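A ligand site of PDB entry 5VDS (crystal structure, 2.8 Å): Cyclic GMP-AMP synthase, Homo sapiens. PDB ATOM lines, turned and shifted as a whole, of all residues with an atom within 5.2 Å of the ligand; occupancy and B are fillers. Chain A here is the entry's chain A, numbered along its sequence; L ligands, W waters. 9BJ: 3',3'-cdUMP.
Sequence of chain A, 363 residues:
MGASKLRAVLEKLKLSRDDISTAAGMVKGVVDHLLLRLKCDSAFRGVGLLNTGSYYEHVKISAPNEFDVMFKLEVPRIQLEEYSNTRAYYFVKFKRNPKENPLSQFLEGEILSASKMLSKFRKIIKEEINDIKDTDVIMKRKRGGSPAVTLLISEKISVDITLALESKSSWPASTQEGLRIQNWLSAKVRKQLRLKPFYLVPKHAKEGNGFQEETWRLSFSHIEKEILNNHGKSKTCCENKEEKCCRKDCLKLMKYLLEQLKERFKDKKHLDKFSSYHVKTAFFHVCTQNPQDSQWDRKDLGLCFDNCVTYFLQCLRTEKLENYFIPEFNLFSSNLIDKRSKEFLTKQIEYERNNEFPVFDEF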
ATOM      1  N   TYR A  89      -8.449  31.232 -14.735  1.00  0.00           N
ATOM      2  CA  TYR A  89      -9.857  30.843 -14.788  1.00  0.00           C
ATOM      3  C   TYR A  89     -10.436  31.088 -16.168  1.00  0.00           C
ATOM      4  O   TYR A  89     -10.205  32.135 -16.777  1.00  0.00           O
ATOM      5  CB  TYR A  89     -10.643  31.610 -13.729  1.00  0.00           C
ATOM      6  CG  TYR A  89     -10.125  31.383 -12.315  1.00  0.00           C
ATOM      7  CD1 TYR A  89      -9.141  32.199 -11.788  1.00  0.00           C
ATOM      8  CD2 TYR A  89     -10.630  30.356 -11.532  1.00  0.00           C
ATOM      9  CE1 TYR A  89      -8.658  31.997 -10.513  1.00  0.00           C
ATOM     10  CE2 TYR A  89     -10.152  30.157 -10.248  1.00  0.00           C
ATOM     11  CZ  TYR A  89      -9.168  30.975  -9.745  1.00  0.00           C
ATOM     12  OH  TYR A  89      -8.690  30.776  -8.462  1.00  0.00           O
ATOM     13  N   PRO A 147     -16.783  22.160  -4.560  1.00  0.00           N
ATOM     14  CA  PRO A 147     -16.000  21.747  -5.728  1.00  0.00           C
ATOM     15  C   PRO A 147     -15.675  20.250  -5.717  1.00  0.00           C
ATOM     16  O   PRO A 147     -15.649  19.623  -6.787  1.00  0.00           O
ATOM     17  CB  PRO A 147     -14.720  22.574  -5.603  1.00  0.00           C
ATOM     18  CG  PRO A 147     -15.128  23.780  -4.819  1.00  0.00           C
ATOM     19  CD  PRO A 147     -16.166  23.287  -3.853  1.00  0.00           C
ATOM     20  N   ALA A 148     -15.447  19.696  -4.536  1.00  0.00           N
ATOM     21  CA  ALA A 148     -15.114  18.284  -4.398  1.00  0.00           C
ATOM     22  C   ALA A 148     -16.289  17.507  -3.789  1.00  0.00           C
ATOM     23  O   ALA A 148     -17.241  18.092  -3.281  1.00  0.00           O
ATOM     24  CB  ALA A 148     -13.868  18.105  -3.549  1.00  0.00           C
ATOM     25  N   THR A 162     -12.589  14.629  -7.167  1.00  0.00           N
ATOM     26  CA  THR A 162     -12.610  15.849  -7.970  1.00  0.00           C
ATOM     27  C   THR A 162     -12.856  15.528  -9.434  1.00  0.00           C
ATOM     28  O   THR A 162     -12.183  14.679 -10.017  1.00  0.00           O
ATOM     29  CB  THR A 162     -11.282  16.631  -7.832  1.00  0.00           C
ATOM     30  OG1 THR A 162     -11.124  17.068  -6.480  1.00  0.00           O
ATOM     31  CG2 THR A 162     -11.277  17.847  -8.749  1.00  0.00           C
ATOM     32  N   VAL A 201     -10.553  22.204 -13.533  1.00  0.00           N
ATOM     33  CA  VAL A 201     -11.376  21.849 -12.381  1.00  0.00           C
ATOM     34  C   VAL A 201     -12.373  22.968 -12.101  1.00  0.00           C
ATOM     35  O   VAL A 201     -12.076  24.139 -12.316  1.00  0.00           O
ATOM     36  CB  VAL A 201     -10.511  21.565 -11.141  1.00  0.00           C
ATOM     37  CG1 VAL A 201      -9.663  20.316 -11.371  1.00  0.00           C
ATOM     38  CG2 VAL A 201      -9.626  22.759 -10.821  1.00  0.00           C
ATOM     39  N   PRO A 202     -13.578  22.603 -11.642  1.00  0.00           N
ATOM     40  CA  PRO A 202     -14.582  23.618 -11.323  1.00  0.00           C
ATOM     41  C   PRO A 202     -14.193  24.466 -10.112  1.00  0.00           C
ATOM     42  O   PRO A 202     -14.136  23.955  -8.990  1.00  0.00           O
ATOM     43  CB  PRO A 202     -15.848  22.794 -11.029  1.00  0.00           C
ATOM     44  CG  PRO A 202     -15.328  21.466 -10.611  1.00  0.00           C
ATOM     45  CD  PRO A 202     -14.085  21.235 -11.410  1.00  0.00           C
ATOM     46  N   LYS A 203     -13.921  25.745 -10.348  1.00  0.00           N
ATOM     47  CA  LYS A 203     -13.523  26.646  -9.264  1.00  0.00           C
ATOM     48  C   LYS A 203     -13.843  28.087  -9.633  1.00  0.00           C
ATOM     49  O   LYS A 203     -13.556  28.541 -10.736  1.00  0.00           O
ATOM     50  CB  LYS A 203     -12.035  26.500  -8.963  1.00  0.00           C
ATOM     51  CG  LYS A 203     -11.599  27.175  -7.678  1.00  0.00           C
ATOM     52  CD  LYS A 203     -12.280  26.542  -6.467  1.00  0.00           C
ATOM     53  CE  LYS A 203     -11.965  27.301  -5.195  1.00  0.00           C
ATOM     54  NZ  LYS A 203     -12.632  26.693  -4.007  1.00  0.00           N
ATOM     55  N   ARG A 217     -10.700  26.391 -13.483  1.00  0.00           N
ATOM     56  CA  ARG A 217      -9.291  26.709 -13.292  1.00  0.00           C
ATOM     57  C   ARG A 217      -8.405  25.639 -13.914  1.00  0.00           C
ATOM     58  O   ARG A 217      -8.714  24.442 -13.870  1.00  0.00           O
ATOM     59  CB  ARG A 217      -8.968  26.846 -11.794  1.00  0.00           C
ATOM     60  CG  ARG A 217      -7.559  27.363 -11.514  1.00  0.00           C
ATOM     61  CD  ARG A 217      -7.246  27.305 -10.030  1.00  0.00           C
ATOM     62  NE  ARG A 217      -7.209  25.929  -9.539  1.00  0.00           N
ATOM     63  CZ  ARG A 217      -7.429  25.576  -8.275  1.00  0.00           C
ATOM     64  NH1 ARG A 217      -7.377  24.303  -7.922  1.00  0.00           N
ATOM     65  NH2 ARG A 217      -7.702  26.504  -7.366  1.00  0.00           N
ATOM     66  N   LEU A 218      -7.295  26.083 -14.499  1.00  0.00           N
ATOM     67  CA  LEU A 218      -6.316  25.172 -15.103  1.00  0.00           C
ATOM     68  C   LEU A 218      -5.712  24.261 -14.049  1.00  0.00           C
ATOM     69  O   LEU A 218      -5.540  24.645 -12.891  1.00  0.00           O
ATOM     70  CB  LEU A 218      -5.214  25.957 -15.806  1.00  0.00           C
ATOM     71  CG  LEU A 218      -5.613  26.810 -17.009  1.00  0.00           C
ATOM     72  CD1 LEU A 218      -4.447  27.666 -17.475  1.00  0.00           C
ATOM     73  CD2 LEU A 218      -6.112  25.927 -18.147  1.00  0.00           C
ATOM     74  N   SER A 219      -5.381  23.040 -14.451  1.00  0.00           N
ATOM     75  CA  SER A 219      -4.788  22.065 -13.555  1.00  0.00           C
ATOM     76  C   SER A 219      -3.773  21.196 -14.292  1.00  0.00           C
ATOM     77  O   SER A 219      -4.042  20.705 -15.405  1.00  0.00           O
ATOM     78  CB  SER A 219      -5.867  21.187 -12.916  1.00  0.00           C
ATOM     79  OG  SER A 219      -5.310  20.333 -11.935  1.00  0.00           O
ATOM     80  N   PHE A 220      -2.611  21.031 -13.670  1.00  0.00           N
ATOM     81  CA  PHE A 220      -1.514  20.250 -14.222  1.00  0.00           C
ATOM     82  C   PHE A 220      -0.949  19.280 -13.180  1.00  0.00           C
ATOM     83  O   PHE A 220       0.257  19.143 -13.051  1.00  0.00           O
ATOM     84  CB  PHE A 220      -0.389  21.165 -14.725  1.00  0.00           C
ATOM     85  CG  PHE A 220      -0.841  22.249 -15.668  1.00  0.00           C
ATOM     86  CD1 PHE A 220      -0.849  22.027 -17.038  1.00  0.00           C
ATOM     87  CD2 PHE A 220      -1.253  23.483 -15.182  1.00  0.00           C
ATOM     88  CE1 PHE A 220      -1.262  23.024 -17.902  1.00  0.00           C
ATOM     89  CE2 PHE A 220      -1.662  24.477 -16.054  1.00  0.00           C
ATOM     90  CZ  PHE A 220      -1.673  24.248 -17.412  1.00  0.00           C
ATOM     91  N   SER A 221      -1.848  18.625 -12.443  1.00  0.00           N
ATOM     92  CA  SER A 221      -1.437  17.716 -11.378  1.00  0.00           C
ATOM     93  C   SER A 221      -0.551  16.596 -11.893  1.00  0.00           C
ATOM     94  O   SER A 221       0.404  16.177 -11.235  1.00  0.00           O
ATOM     95  CB  SER A 221      -2.673  17.131 -10.684  1.00  0.00           C
ATOM     96  OG  SER A 221      -3.477  18.161 -10.137  1.00  0.00           O
ATOM     97  N   GLU A 224       2.932  17.879 -12.425  1.00  0.00           N
ATOM     98  CA  GLU A 224       3.588  18.042 -11.133  1.00  0.00           C
ATOM     99  C   GLU A 224       4.088  16.697 -10.605  1.00  0.00           C
ATOM    100  O   GLU A 224       5.226  16.584 -10.136  1.00  0.00           O
ATOM    101  CB  GLU A 224       2.620  18.684 -10.134  1.00  0.00           C
ATOM    102  CG  GLU A 224       2.153  20.060 -10.542  1.00  0.00           C
ATOM    103  CD  GLU A 224       0.910  20.506  -9.796  1.00  0.00           C
ATOM    104  OE1 GLU A 224       0.374  19.715  -8.995  1.00  0.00           O
ATOM    105  OE2 GLU A 224       0.472  21.655 -10.006  1.00  0.00           O
ATOM    106  N   SER A 275      -1.743  26.184   2.367  1.00  0.00           N
ATOM    107  CA  SER A 275      -1.840  24.744   2.149  1.00  0.00           C
ATOM    108  C   SER A 275      -0.604  24.186   1.446  1.00  0.00           C
ATOM    109  O   SER A 275       0.317  24.928   1.095  1.00  0.00           O
ATOM    110  CB  SER A 275      -3.086  24.416   1.328  1.00  0.00           C
ATOM    111  OG  SER A 275      -2.979  24.938   0.017  1.00  0.00           O
ATOM    112  N   SER A 276      -0.603  22.874   1.247  1.00  0.00           N
ATOM    113  CA  SER A 276       0.552  22.163   0.735  1.00  0.00           C
ATOM    114  C   SER A 276       0.944  22.581  -0.685  1.00  0.00           C
ATOM    115  O   SER A 276       2.104  22.454  -1.062  1.00  0.00           O
ATOM    116  CB  SER A 276       0.300  20.649   0.766  1.00  0.00           C
ATOM    117  OG  SER A 276      -0.835  20.314  -0.001  1.00  0.00           O
ATOM    118  N   TYR A 277      -0.021  23.077  -1.463  1.00  0.00           N
ATOM    119  CA  TYR A 277       0.264  23.450  -2.840  1.00  0.00           C
ATOM    120  C   TYR A 277       1.170  24.678  -2.933  1.00  0.00           C
ATOM    121  O   TYR A 277       1.970  24.788  -3.862  1.00  0.00           O
ATOM    122  CB  TYR A 277      -1.027  23.703  -3.618  1.00  0.00           C
ATOM    123  CG  TYR A 277      -0.785  23.902  -5.101  1.00  0.00           C
ATOM    124  CD1 TYR A 277      -0.660  22.824  -5.954  1.00  0.00           C
ATOM    125  CD2 TYR A 277      -0.654  25.179  -5.632  1.00  0.00           C
ATOM    126  CE1 TYR A 277      -0.433  23.001  -7.310  1.00  0.00           C
ATOM    127  CE2 TYR A 277      -0.423  25.379  -6.982  1.00  0.00           C
ATOM    128  CZ  TYR A 277      -0.314  24.286  -7.815  1.00  0.00           C
ATOM    129  OH  TYR A 277      -0.082  24.466  -9.159  1.00  0.00           O
ATOM    130  N   HIS A 278       1.026  25.587  -1.981  1.00  0.00           N
ATOM    131  CA  HIS A 278       1.912  26.750  -1.915  1.00  0.00           C
ATOM    132  C   HIS A 278       3.338  26.274  -1.705  1.00  0.00           C
ATOM    133  O   HIS A 278       4.273  26.679  -2.407  1.00  0.00           O
ATOM    134  CB  HIS A 278       1.494  27.688  -0.791  1.00  0.00           C
ATOM    135  CG  HIS A 278       0.118  28.274  -0.965  1.00  0.00           C
ATOM    136  ND1 HIS A 278      -0.788  28.362   0.072  1.00  0.00           N
ATOM    137  CD2 HIS A 278      -0.493  28.794  -2.053  1.00  0.00           C
ATOM    138  CE1 HIS A 278      -1.903  28.908  -0.368  1.00  0.00           C
ATOM    139  NE2 HIS A 278      -1.756  29.176  -1.653  1.00  0.00           N
ATOM    140  N   ASN A 323       2.227  30.929  -9.704  1.00  0.00           N
ATOM    141  CA  ASN A 323       1.904  29.580 -10.114  1.00  0.00           C
ATOM    142  C   ASN A 323       2.994  29.092 -11.056  1.00  0.00           C
ATOM    143  O   ASN A 323       3.397  29.803 -11.976  1.00  0.00           O
ATOM    144  CB  ASN A 323       0.529  29.528 -10.781  1.00  0.00           C
ATOM    145  CG  ASN A 323       0.103  28.122 -11.153  1.00  0.00           C
ATOM    146  OD1 ASN A 323       0.595  27.546 -12.122  1.00  0.00           O
ATOM    147  ND2 ASN A 323      -0.830  27.571 -10.384  1.00  0.00           N
ATOM    148  N   PHE A 329      -0.198  34.439 -12.417  1.00  0.00           N
ATOM    149  CA  PHE A 329      -1.204  34.089 -11.410  1.00  0.00           C
ATOM    150  C   PHE A 329      -0.536  33.963 -10.036  1.00  0.00           C
ATOM    151  O   PHE A 329       0.158  32.990  -9.758  1.00  0.00           O
ATOM    152  CB  PHE A 329      -1.918  32.786 -11.800  1.00  0.00           C
ATOM    153  CG  PHE A 329      -2.879  32.277 -10.770  1.00  0.00           C
ATOM    154  CD1 PHE A 329      -3.755  33.144 -10.127  1.00  0.00           C
ATOM    155  CD2 PHE A 329      -2.920  30.935 -10.451  1.00  0.00           C
ATOM    156  CE1 PHE A 329      -4.646  32.666  -9.177  1.00  0.00           C
ATOM    157  CE2 PHE A 329      -3.807  30.454  -9.509  1.00  0.00           C
ATOM    158  CZ  PHE A 329      -4.670  31.320  -8.872  1.00  0.00           C
ATOM    159  N   LEU A 331      -0.352  33.352  -6.187  1.00  0.00           N
ATOM    160  CA  LEU A 331      -1.042  32.628  -5.124  1.00  0.00           C
ATOM    161  C   LEU A 331      -1.034  33.393  -3.804  1.00  0.00           C
ATOM    162  O   LEU A 331      -1.853  33.130  -2.919  1.00  0.00           O
ATOM    163  CB  LEU A 331      -0.393  31.248  -4.916  1.00  0.00           C
ATOM    164  CG  LEU A 331      -0.290  30.332  -6.138  1.00  0.00           C
ATOM    165  CD1 LEU A 331       0.296  28.990  -5.741  1.00  0.00           C
ATOM    166  CD2 LEU A 331      -1.650  30.161  -6.785  1.00  0.00           C
ATOM    167  N   LEU A 336      -6.135  37.358  -2.299  1.00  0.00           N
ATOM    168  CA  LEU A 336      -6.347  35.979  -1.868  1.00  0.00           C
ATOM    169  C   LEU A 336      -6.052  35.818  -0.372  1.00  0.00           C
ATOM    170  O   LEU A 336      -6.867  35.275   0.371  1.00  0.00           O
ATOM    171  CB  LEU A 336      -5.481  35.023  -2.683  1.00  0.00           C
ATOM    172  CG  LEU A 336      -5.775  34.952  -4.176  1.00  0.00           C
ATOM    173  CD1 LEU A 336      -4.932  33.873  -4.850  1.00  0.00           C
ATOM    174  CD2 LEU A 336      -7.252  34.688  -4.415  1.00  0.00           C
HETATM  175  C10 9BJ L   1      -9.997  22.492  -2.430  1.00  0.00           C
HETATM  176  C13 9BJ L   1     -10.637  22.659  -6.292  1.00  0.00           C
HETATM  177  C21 9BJ L   1      -5.584  26.974  -4.273  1.00  0.00           C
HETATM  178  C22 9BJ L   1      -4.575  26.996  -3.504  1.00  0.00           C
HETATM  179  O01 9BJ L   1      -8.986  27.514  -4.976  1.00  0.00           O
HETATM  180  P02 9BJ L   1      -8.223  27.259  -3.690  1.00  0.00           P
HETATM  181  O03 9BJ L   1      -8.335  25.673  -3.136  1.00  0.00           O
HETATM  182  C04 9BJ L   1      -8.486  25.455  -1.731  1.00  0.00           C
HETATM  183  C05 9BJ L   1      -8.737  24.116  -1.490  1.00  0.00           C
HETATM  184  C06 9BJ L   1      -7.744  23.163  -2.350  1.00  0.00           C
HETATM  185  O07 9BJ L   1      -6.440  22.966  -1.628  1.00  0.00           O
HETATM  186  C08 9BJ L   1      -8.366  22.094  -2.434  1.00  0.00           C
HETATM  187  O09 9BJ L   1      -8.054  21.230  -1.280  1.00  0.00           O
HETATM  188  N11 9BJ L   1     -10.374  22.106  -3.810  1.00  0.00           N
HETATM  189  C12 9BJ L   1     -10.246  23.061  -4.899  1.00  0.00           C
HETATM  190  C14 9BJ L   1     -11.161  21.286  -6.548  1.00  0.00           C
HETATM  191  N15 9BJ L   1     -11.290  20.340  -5.462  1.00  0.00           N
HETATM  192  C16 9BJ L   1     -10.904  20.738  -4.082  1.00  0.00           C
HETATM  193  O17 9BJ L   1     -11.009  19.953  -3.183  1.00  0.00           O
HETATM  194  O18 9BJ L   1     -11.478  20.972  -7.657  1.00  0.00           O
HETATM  195  O19 9BJ L   1     -10.110  23.723  -1.974  1.00  0.00           O
HETATM  196  O20 9BJ L   1      -6.668  27.851  -3.720  1.00  0.00           O
HETATM  197  C23 9BJ L   1      -4.619  25.808  -2.558  1.00  0.00           C
HETATM  198  O24 9BJ L   1      -4.937  24.634  -3.304  1.00  0.00           O
HETATM  199  P25 9BJ L   1      -5.040  23.161  -2.506  1.00  0.00           P
HETATM  200  O26 9BJ L   1      -4.696  21.973  -3.382  1.00  0.00           O
HETATM  201  O27 9BJ L   1      -3.935  23.194  -1.466  1.00  0.00           O
HETATM  202  O28 9BJ L   1      -3.216  26.892  -4.482  1.00  0.00           O
HETATM  203  C29 9BJ L   1      -3.596  27.049  -5.718  1.00  0.00           C
HETATM  204  N30 9BJ L   1      -3.702  25.913  -6.674  1.00  0.00           N
HETATM  205  C31 9BJ L   1      -3.564  26.144  -8.135  1.00  0.00           C
HETATM  206  N32 9BJ L   1      -3.665  24.996  -9.096  1.00  0.00           N
HETATM  207  C33 9BJ L   1      -3.898  23.646  -8.603  1.00  0.00           C
HETATM  208  C34 9BJ L   1      -4.040  23.409  -7.130  1.00  0.00           C
HETATM  209  C35 9BJ L   1      -3.935  24.564  -6.181  1.00  0.00           C
HETATM  210  O36 9BJ L   1      -3.981  22.738  -9.353  1.00  0.00           O
HETATM  211  O37 9BJ L   1      -3.378  27.241  -8.552  1.00  0.00           O
HETATM  212  C38 9BJ L   1      -5.057  27.554  -5.644  1.00  0.00           C
HETATM  213  O39 9BJ L   1      -5.091  28.891  -5.617  1.00  0.00           O
HETATM  214  O40 9BJ L   1      -8.927  28.080  -2.643  1.00  0.00           O
HETATM  215  O   HOH W   1      -2.432  25.538 -11.442  1.00  0.00           O
HETATM  216  O   HOH W   2      -4.058  30.916  -3.014  1.00  0.00           O
HETATM  217  O   HOH W   3      -2.184  22.975 -11.293  1.00  0.00           O
HETATM  218  O   HOH W   4      -6.483  23.541 -10.445  1.00  0.00           O
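The side-chain hydroxyl (OG) of Ser 275 sits at hydrogen-bond distance from an oxygen (O27) of the ligand.
An oxygen (O01) of the ligand lies within salt-bridge range of the guanidinium group (NH2) of Arg 217 (2.9 Å).
An oxygen (O01) of the ligand is in salt-bridge range of the side-chain amino group of Lys 203 (3.9 Å).
ND2 of Asn 323 is in hydrogen-bond range of O37 of the ligand (3.2 Å).
A nitrogen (N15) of the ligand sits at hydrogen-bond distance from the side-chain hydroxyl (OG1) of Thr 162 (3.4 Å).
N of Ser 275 lies within hydrogen-bond range of ND1 of His 278, 3.3 Å away.
The backbone carbonyl oxygen (O) of Val 201 lies within hydrogen-bond range of the backbone NH (N) of Arg 217.
OH of Tyr 277 sits at hydrogen-bond distance from ND2 of Asn 323 (3.4 Å).
N of Asn 323 sits at hydrogen-bond distance from O of Phe 329 (2.9 Å).
OH of Tyr 277 is in hydrogen-bond range of OE2 of Glu 224 (3.0 Å).
The side-chain hydroxyl (OG) of Ser 219 sits at hydrogen-bond distance from the side-chain hydroxyl (OG) of Ser 221 (3.4 Å).
CB of Pro 147 touches C14 of the ligand, at 3.9 Å.
Ala 148 touches the ligand (CB to O17, 3.4 Å).
Val 201 touches the ligand (CB to O18, 3.7 Å).
OG of Ser 219 touches O36 of the ligand (3.8 Å).
Tyr 277 touches the ligand.
His 278 touches the ligand (NE2 to O28, 3.9 Å).
CE2 of Phe 329 touches O37 of the ligand, 3.4 Å away.
Leu 331 touches the ligand (CD2 to C29, 3.8 Å).
Of the 21 residues printed, 13 come within 4 Å of the ligand.
The nearest printed residue that does not touch the ligand is Pro 202 (4.2 Å).
Water W3 lies within hydrogen-bond range of an oxygen (O36) of the ligand, the backbone NH (N) of Phe 220, the side-chain carboxylate (OE2) of Glu 224 and the side-chain hydroxyl (OH) of Tyr 277.
Water W1 lies within hydrogen-bond range of N32 of the ligand (2.7 Å), ND2 of Asn 323 (2.8 Å) and OH of Tyr 277 (3.4 Å).
Water W4 lies within hydrogen-bond range of NE of Arg 217 (2.7 Å), O of Leu 218 (2.8 Å) and O36 of the ligand (2.8 Å).
Water W2 lies within hydrogen-bond range of the backbone carbonyl oxygen of Leu 331, a ring nitrogen (NE2) of His 278 and an oxygen (O39) of the ligand.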
